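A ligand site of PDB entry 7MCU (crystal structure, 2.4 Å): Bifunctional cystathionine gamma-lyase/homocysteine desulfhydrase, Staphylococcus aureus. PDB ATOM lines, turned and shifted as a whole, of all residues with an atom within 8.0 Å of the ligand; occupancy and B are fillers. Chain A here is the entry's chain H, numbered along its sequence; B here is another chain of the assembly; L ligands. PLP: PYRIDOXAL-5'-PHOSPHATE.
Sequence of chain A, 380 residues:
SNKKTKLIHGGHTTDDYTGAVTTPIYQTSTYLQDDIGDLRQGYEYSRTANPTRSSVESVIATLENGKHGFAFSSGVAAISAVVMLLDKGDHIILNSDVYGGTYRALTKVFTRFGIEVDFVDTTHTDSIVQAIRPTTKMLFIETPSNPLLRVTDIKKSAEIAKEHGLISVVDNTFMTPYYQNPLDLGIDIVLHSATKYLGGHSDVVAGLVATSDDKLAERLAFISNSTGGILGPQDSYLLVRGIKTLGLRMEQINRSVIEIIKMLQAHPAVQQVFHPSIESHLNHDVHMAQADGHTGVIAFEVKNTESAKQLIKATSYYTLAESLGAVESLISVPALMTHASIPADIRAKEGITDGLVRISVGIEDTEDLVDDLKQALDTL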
ATOM      1  N   SER A   1     -25.297 -25.876  15.972  1.00  0.00           N
ATOM      2  CA  SER A   1     -24.085 -25.063  16.067  1.00  0.00           C
ATOM      3  C   SER A   1     -23.743 -24.459  14.694  1.00  0.00           C
ATOM      4  O   SER A   1     -24.333 -23.461  14.308  1.00  0.00           O
ATOM      5  CB  SER A   1     -22.922 -25.899  16.609  1.00  0.00           C
ATOM      6  OG  SER A   1     -21.772 -25.095  16.866  1.00  0.00           O
ATOM      7  N   ASN A   2     -22.799 -25.078  13.968  1.00  0.00           N
ATOM      8  CA  ASN A   2     -22.419 -24.608  12.633  1.00  0.00           C
ATOM      9  C   ASN A   2     -23.491 -24.998  11.609  1.00  0.00           C
ATOM     10  O   ASN A   2     -24.354 -25.844  11.854  1.00  0.00           O
ATOM     11  CB  ASN A   2     -21.064 -25.173  12.227  1.00  0.00           C
ATOM     12  CG  ASN A   2     -19.924 -24.531  12.986  1.00  0.00           C
ATOM     13  OD1 ASN A   2     -20.026 -23.394  13.451  1.00  0.00           O
ATOM     14  ND2 ASN A   2     -18.807 -25.245  13.105  1.00  0.00           N
ATOM     15  N   LYS A   3     -23.413 -24.359  10.419  1.00  0.00           N
ATOM     16  CA  LYS A   3     -24.529 -24.390   9.475  1.00  0.00           C
ATOM     17  C   LYS A   3     -24.820 -25.801   8.959  1.00  0.00           C
ATOM     18  O   LYS A   3     -25.989 -26.224   8.870  1.00  0.00           O
ATOM     19  CB  LYS A   3     -24.252 -23.454   8.293  1.00  0.00           C
ATOM     20  CG  LYS A   3     -23.719 -22.095   8.673  1.00  0.00           C
ATOM     21  CD  LYS A   3     -23.883 -21.087   7.526  1.00  0.00           C
ATOM     22  CE  LYS A   3     -22.722 -21.173   6.522  1.00  0.00           C
ATOM     23  NZ  LYS A   3     -22.668 -20.037   5.560  1.00  0.00           N
ATOM     24  N   LYS A   4     -23.787 -26.549   8.575  1.00  0.00           N
ATOM     25  CA  LYS A   4     -24.036 -27.880   8.030  1.00  0.00           C
ATOM     26  C   LYS A   4     -24.695 -28.781   9.060  1.00  0.00           C
ATOM     27  O   LYS A   4     -25.453 -29.688   8.712  1.00  0.00           O
ATOM     28  CB  LYS A   4     -22.748 -28.485   7.494  1.00  0.00           C
ATOM     29  CG  LYS A   4     -22.274 -27.786   6.239  1.00  0.00           C
ATOM     30  CD  LYS A   4     -21.145 -28.537   5.582  1.00  0.00           C
ATOM     31  CE  LYS A   4     -19.928 -27.644   5.408  1.00  0.00           C
ATOM     32  NZ  LYS A   4     -18.907 -28.280   4.541  1.00  0.00           N
ATOM     33  N   THR A   5     -24.443 -28.527  10.356  1.00  0.00           N
ATOM     34  CA  THR A   5     -25.112 -29.270  11.423  1.00  0.00           C
ATOM     35  C   THR A   5     -26.562 -28.842  11.595  1.00  0.00           C
ATOM     36  O   THR A   5     -27.468 -29.686  11.693  1.00  0.00           O
ATOM     37  CB  THR A   5     -24.337 -29.079  12.736  1.00  0.00           C
ATOM     38  OG1 THR A   5     -22.972 -29.475  12.541  1.00  0.00           O
ATOM     39  CG2 THR A   5     -24.949 -29.895  13.860  1.00  0.00           C
ATOM     40  N   LYS A   6     -26.782 -27.526  11.622  1.00  0.00           N
ATOM     41  CA  LYS A   6     -28.135 -26.967  11.721  1.00  0.00           C
ATOM     42  C   LYS A   6     -29.027 -27.453  10.581  1.00  0.00           C
ATOM     43  O   LYS A   6     -30.221 -27.687  10.799  1.00  0.00           O
ATOM     44  CB  LYS A   6     -28.030 -25.445  11.755  1.00  0.00           C
ATOM     45  CG  LYS A   6     -29.313 -24.686  12.038  1.00  0.00           C
ATOM     46  CD  LYS A   6     -29.009 -23.197  12.087  1.00  0.00           C
ATOM     47  CE  LYS A   6     -30.251 -22.322  12.127  1.00  0.00           C
ATOM     48  NZ  LYS A   6     -29.912 -20.862  12.173  1.00  0.00           N
ATOM     49  N   LEU A   7     -28.469 -27.608   9.377  1.00  0.00           N
ATOM     50  CA  LEU A   7     -29.222 -28.170   8.259  1.00  0.00           C
ATOM     51  C   LEU A   7     -29.740 -29.570   8.557  1.00  0.00           C
ATOM     52  O   LEU A   7     -30.816 -29.948   8.080  1.00  0.00           O
ATOM     53  CB  LEU A   7     -28.360 -28.203   7.000  1.00  0.00           C
ATOM     54  CG  LEU A   7     -28.247 -26.857   6.277  1.00  0.00           C
ATOM     55  CD1 LEU A   7     -27.241 -26.983   5.168  1.00  0.00           C
ATOM     56  CD2 LEU A   7     -29.616 -26.416   5.760  1.00  0.00           C
ATOM     57  N   ILE A   8     -28.992 -30.362   9.314  1.00  0.00           N
ATOM     58  CA  ILE A   8     -29.379 -31.747   9.549  1.00  0.00           C
ATOM     59  C   ILE A   8     -30.286 -31.860  10.757  1.00  0.00           C
ATOM     60  O   ILE A   8     -31.218 -32.673  10.788  1.00  0.00           O
ATOM     61  CB  ILE A   8     -28.119 -32.611   9.696  1.00  0.00           C
ATOM     62  CG1 ILE A   8     -27.259 -32.495   8.432  1.00  0.00           C
ATOM     63  CG2 ILE A   8     -28.466 -34.074  10.026  1.00  0.00           C
ATOM     64  CD1 ILE A   8     -28.037 -32.612   7.163  1.00  0.00           C
ATOM     65  N   HIS A   9     -30.050 -31.043  11.783  1.00  0.00           N
ATOM     66  CA  HIS A   9     -30.763 -31.222  13.034  1.00  0.00           C
ATOM     67  C   HIS A   9     -31.739 -30.102  13.367  1.00  0.00           C
ATOM     68  O   HIS A   9     -32.514 -30.237  14.319  1.00  0.00           O
ATOM     69  CB  HIS A   9     -29.748 -31.448  14.154  1.00  0.00           C
ATOM     70  CG  HIS A   9     -28.928 -32.685  13.957  1.00  0.00           C
ATOM     71  ND1 HIS A   9     -29.432 -33.943  14.202  1.00  0.00           N
ATOM     72  CD2 HIS A   9     -27.682 -32.866  13.467  1.00  0.00           C
ATOM     73  CE1 HIS A   9     -28.510 -34.846  13.895  1.00  0.00           C
ATOM     74  NE2 HIS A   9     -27.437 -34.216  13.457  1.00  0.00           N
ATOM     75  N   GLY A  10     -31.742 -29.003  12.610  1.00  0.00           N
ATOM     76  CA  GLY A  10     -32.725 -27.953  12.841  1.00  0.00           C
ATOM     77  C   GLY A  10     -34.091 -28.301  12.289  1.00  0.00           C
ATOM     78  O   GLY A  10     -34.224 -28.941  11.250  1.00  0.00           O
ATOM     79  N   GLY A  11     -35.120 -27.853  12.987  1.00  0.00           N
ATOM     80  CA  GLY A  11     -36.480 -28.204  12.635  1.00  0.00           C
ATOM     81  C   GLY A  11     -36.884 -29.532  13.261  1.00  0.00           C
ATOM     82  O   GLY A  11     -36.096 -30.216  13.918  1.00  0.00           O
ATOM     83  N   THR A  62     -36.650 -22.386  11.178  1.00  0.00           N
ATOM     84  CA  THR A  62     -35.388 -22.584  11.879  1.00  0.00           C
ATOM     85  C   THR A  62     -34.203 -22.049  11.081  1.00  0.00           C
ATOM     86  O   THR A  62     -33.340 -21.343  11.617  1.00  0.00           O
ATOM     87  CB  THR A  62     -35.182 -24.078  12.196  1.00  0.00           C
ATOM     88  OG1 THR A  62     -36.124 -24.476  13.195  1.00  0.00           O
ATOM     89  CG2 THR A  62     -33.770 -24.344  12.692  1.00  0.00           C
ATOM     90  N   LEU A  63     -34.149 -22.371   9.786  1.00  0.00           N
ATOM     91  CA  LEU A  63     -33.016 -21.973   8.951  1.00  0.00           C
ATOM     92  C   LEU A  63     -32.924 -20.461   8.755  1.00  0.00           C
ATOM     93  O   LEU A  63     -31.829 -19.924   8.546  1.00  0.00           O
ATOM     94  CB  LEU A  63     -33.103 -22.690   7.596  1.00  0.00           C
ATOM     95  CG  LEU A  63     -32.908 -24.205   7.634  1.00  0.00           C
ATOM     96  CD1 LEU A  63     -32.968 -24.775   6.227  1.00  0.00           C
ATOM     97  CD2 LEU A  63     -31.581 -24.551   8.318  1.00  0.00           C
ATOM     98  N   GLU A  64     -34.052 -19.757   8.813  1.00  0.00           N
ATOM     99  CA  GLU A  64     -34.048 -18.298   8.684  1.00  0.00           C
ATOM    100  C   GLU A  64     -34.089 -17.597  10.024  1.00  0.00           C
ATOM    101  O   GLU A  64     -34.295 -16.382  10.058  1.00  0.00           O
ATOM    102  CB  GLU A  64     -35.223 -17.848   7.806  1.00  0.00           C
ATOM    103  CG  GLU A  64     -35.070 -18.191   6.329  1.00  0.00           C
ATOM    104  CD  GLU A  64     -34.027 -17.322   5.614  1.00  0.00           C
ATOM    105  OE1 GLU A  64     -33.145 -16.734   6.284  1.00  0.00           O
ATOM    106  OE2 GLU A  64     -34.089 -17.227   4.369  1.00  0.00           O
ATOM    107  N   ASN A  65     -33.907 -18.334  11.128  1.00  0.00           N
ATOM    108  CA  ASN A  65     -33.982 -17.794  12.490  1.00  0.00           C
ATOM    109  C   ASN A  65     -35.277 -17.030  12.728  1.00  0.00           C
ATOM    110  O   ASN A  65     -35.295 -15.985  13.401  1.00  0.00           O
ATOM    111  CB  ASN A  65     -32.776 -16.924  12.826  1.00  0.00           C
ATOM    112  CG  ASN A  65     -31.479 -17.664  12.681  1.00  0.00           C
ATOM    113  OD1 ASN A  65     -31.386 -18.859  13.005  1.00  0.00           O
ATOM    114  ND2 ASN A  65     -30.459 -16.981  12.152  1.00  0.00           N
ATOM    115  N   ASN A 181     -29.490 -14.181   5.781  1.00  0.00           N
ATOM    116  CA  ASN A 181     -30.636 -14.304   6.683  1.00  0.00           C
ATOM    117  C   ASN A 181     -31.272 -12.944   6.925  1.00  0.00           C
ATOM    118  O   ASN A 181     -30.944 -12.255   7.895  1.00  0.00           O
ATOM    119  CB  ASN A 181     -30.216 -14.991   7.980  1.00  0.00           C
ATOM    120  CG  ASN A 181     -29.668 -16.394   7.727  1.00  0.00           C
ATOM    121  OD1 ASN A 181     -28.489 -16.657   7.947  1.00  0.00           O
ATOM    122  ND2 ASN A 181     -30.523 -17.277   7.225  1.00  0.00           N
ATOM    123  N   ASP A 184     -32.507 -11.725  10.377  1.00  0.00           N
ATOM    124  CA  ASP A 184     -31.476 -11.320  11.311  1.00  0.00           C
ATOM    125  C   ASP A 184     -31.077  -9.866  11.136  1.00  0.00           C
ATOM    126  O   ASP A 184     -30.507  -9.280  12.061  1.00  0.00           O
ATOM    127  CB  ASP A 184     -30.226 -12.186  11.122  1.00  0.00           C
ATOM    128  CG  ASP A 184     -30.346 -13.547  11.766  1.00  0.00           C
ATOM    129  OD1 ASP A 184     -31.328 -13.774  12.515  1.00  0.00           O
ATOM    130  OD2 ASP A 184     -29.453 -14.396  11.528  1.00  0.00           O
ATOM    131  N   SER B 316     -24.612 -34.840  21.349  1.00  0.00           N
ATOM    132  CA  SER B 316     -25.749 -34.068  20.845  1.00  0.00           C
ATOM    133  C   SER B 316     -26.102 -34.384  19.387  1.00  0.00           C
ATOM    134  O   SER B 316     -27.285 -34.372  19.027  1.00  0.00           O
ATOM    135  CB  SER B 316     -25.491 -32.561  20.974  1.00  0.00           C
ATOM    136  OG  SER B 316     -24.947 -32.222  22.234  1.00  0.00           O
ATOM    137  N   TYR B 317     -25.108 -34.688  18.544  1.00  0.00           N
ATOM    138  CA  TYR B 317     -25.323 -34.857  17.120  1.00  0.00           C
ATOM    139  C   TYR B 317     -25.186 -36.311  16.647  1.00  0.00           C
ATOM    140  O   TYR B 317     -25.173 -36.550  15.433  1.00  0.00           O
ATOM    141  CB  TYR B 317     -24.346 -33.961  16.355  1.00  0.00           C
ATOM    142  CG  TYR B 317     -24.387 -32.524  16.840  1.00  0.00           C
ATOM    143  CD1 TYR B 317     -25.599 -31.850  16.930  1.00  0.00           C
ATOM    144  CD2 TYR B 317     -23.225 -31.861  17.231  1.00  0.00           C
ATOM    145  CE1 TYR B 317     -25.656 -30.548  17.389  1.00  0.00           C
ATOM    146  CE2 TYR B 317     -23.288 -30.540  17.690  1.00  0.00           C
ATOM    147  CZ  TYR B 317     -24.512 -29.892  17.771  1.00  0.00           C
ATOM    148  OH  TYR B 317     -24.604 -28.592  18.219  1.00  0.00           O
ATOM    149  N   GLU B 364     -23.007 -33.652   8.920  1.00  0.00           N
ATOM    150  CA  GLU B 364     -22.960 -32.473   9.774  1.00  0.00           C
ATOM    151  C   GLU B 364     -21.599 -31.802   9.648  1.00  0.00           C
ATOM    152  O   GLU B 364     -20.661 -32.324   9.051  1.00  0.00           O
ATOM    153  CB  GLU B 364     -23.235 -32.836  11.230  1.00  0.00           C
ATOM    154  CG  GLU B 364     -24.618 -33.405  11.469  1.00  0.00           C
ATOM    155  CD  GLU B 364     -24.614 -34.927  11.534  1.00  0.00           C
ATOM    156  OE1 GLU B 364     -23.651 -35.554  11.052  1.00  0.00           O
ATOM    157  OE2 GLU B 364     -25.591 -35.499  12.063  1.00  0.00           O
ATOM    158  N   ASP B 368     -18.182 -29.747  14.477  1.00  0.00           N
ATOM    159  CA  ASP B 368     -19.238 -30.124  15.413  1.00  0.00           C
ATOM    160  C   ASP B 368     -19.177 -31.618  15.735  1.00  0.00           C
ATOM    161  O   ASP B 368     -19.276 -32.009  16.905  1.00  0.00           O
ATOM    162  CB  ASP B 368     -20.603 -29.736  14.846  1.00  0.00           C
ATOM    163  CG  ASP B 368     -20.850 -28.237  14.902  1.00  0.00           C
ATOM    164  OD1 ASP B 368     -20.158 -27.536  15.666  1.00  0.00           O
ATOM    165  OD2 ASP B 368     -21.747 -27.766  14.171  1.00  0.00           O
HETATM  166  N1  PLP L   1     -30.526 -25.821  15.697  1.00  0.00           N
HETATM  167  C2  PLP L   1     -29.614 -26.809  15.602  1.00  0.00           C
HETATM  168  C2A PLP L   1     -30.101 -28.199  15.376  1.00  0.00           C
HETATM  169  C3  PLP L   1     -28.260 -26.540  15.703  1.00  0.00           C
HETATM  170  O3  PLP L   1     -27.374 -27.580  15.603  1.00  0.00           O
HETATM  171  C4  PLP L   1     -27.815 -25.240  15.922  1.00  0.00           C
HETATM  172  C4A PLP L   1     -26.367 -24.926  16.042  1.00  0.00           C
HETATM  173  C5  PLP L   1     -28.792 -24.202  16.025  1.00  0.00           C
HETATM  174  C6  PLP L   1     -30.116 -24.566  15.905  1.00  0.00           C
HETATM  175  C5A PLP L   1     -28.436 -22.773  16.272  1.00  0.00           C
HETATM  176  O4P PLP L   1     -28.216 -22.094  15.043  1.00  0.00           O
HETATM  177  P   PLP L   1     -27.812 -20.536  15.062  1.00  0.00           P
HETATM  178  O1P PLP L   1     -29.042 -19.703  15.374  1.00  0.00           O
HETATM  179  O2P PLP L   1     -26.760 -20.355  16.137  1.00  0.00           O
HETATM  180  O3P PLP L   1     -27.251 -20.160  13.711  1.00  0.00           O
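The side-chain hydroxyl (OG1) of Thr 5 lies within hydrogen-bond range of the side-chain carboxylate (OD2) of Asp 368 of chain B, 2.7 Å away.
OG of Ser 1 is in hydrogen-bond range of OD1 of Asp 368 of chain B (3.2 Å).
NE2 of His 9 is in hydrogen-bond range of OE2 of Glu 364 of chain B (2.6 Å).
The side-chain carboxylate of Asp 184 sits at hydrogen-bond distance from the side-chain amide nitrogen of Asn 65 (2.8 Å).
The side-chain amino group (NZ) of Lys 6 lies within hydrogen-bond range of the side-chain amide oxygen (OD1) of Asn 65.
The side-chain amide oxygen (OD1) of Asn 65 sits close to the backbone carbonyl oxygen (O) of Thr 62 (3.5 Å).
Thr 5 touches the ligand.
C of His 9 touches C2A of the ligand, 3.2 Å away.
Gly 10 touches the ligand.
Tyr 317 of chain B touches the ligand (CE1 to O3, 3.9 Å).
Hydrophobic or aromatic side chains that line the ligand: His 9 and Tyr 317 of chain B.
Of the 21 residues printed, 7 come within 4 Å of the ligand.
The nearest printed residue that does not touch the ligand is Asn 2 (4.1 Å).
A carbon (C4A) of the ligand is bonded to the backbone NH (N) of Ser 1, 1.4 Å away.
An oxygen (O1P) of the ligand sits close to the side-chain amide oxygen (OD1) of Asn 65.
An oxygen (O3P) of the ligand lies within salt-bridge range of the side-chain amino group (NZ) of Lys 6, 3.2 Å away.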
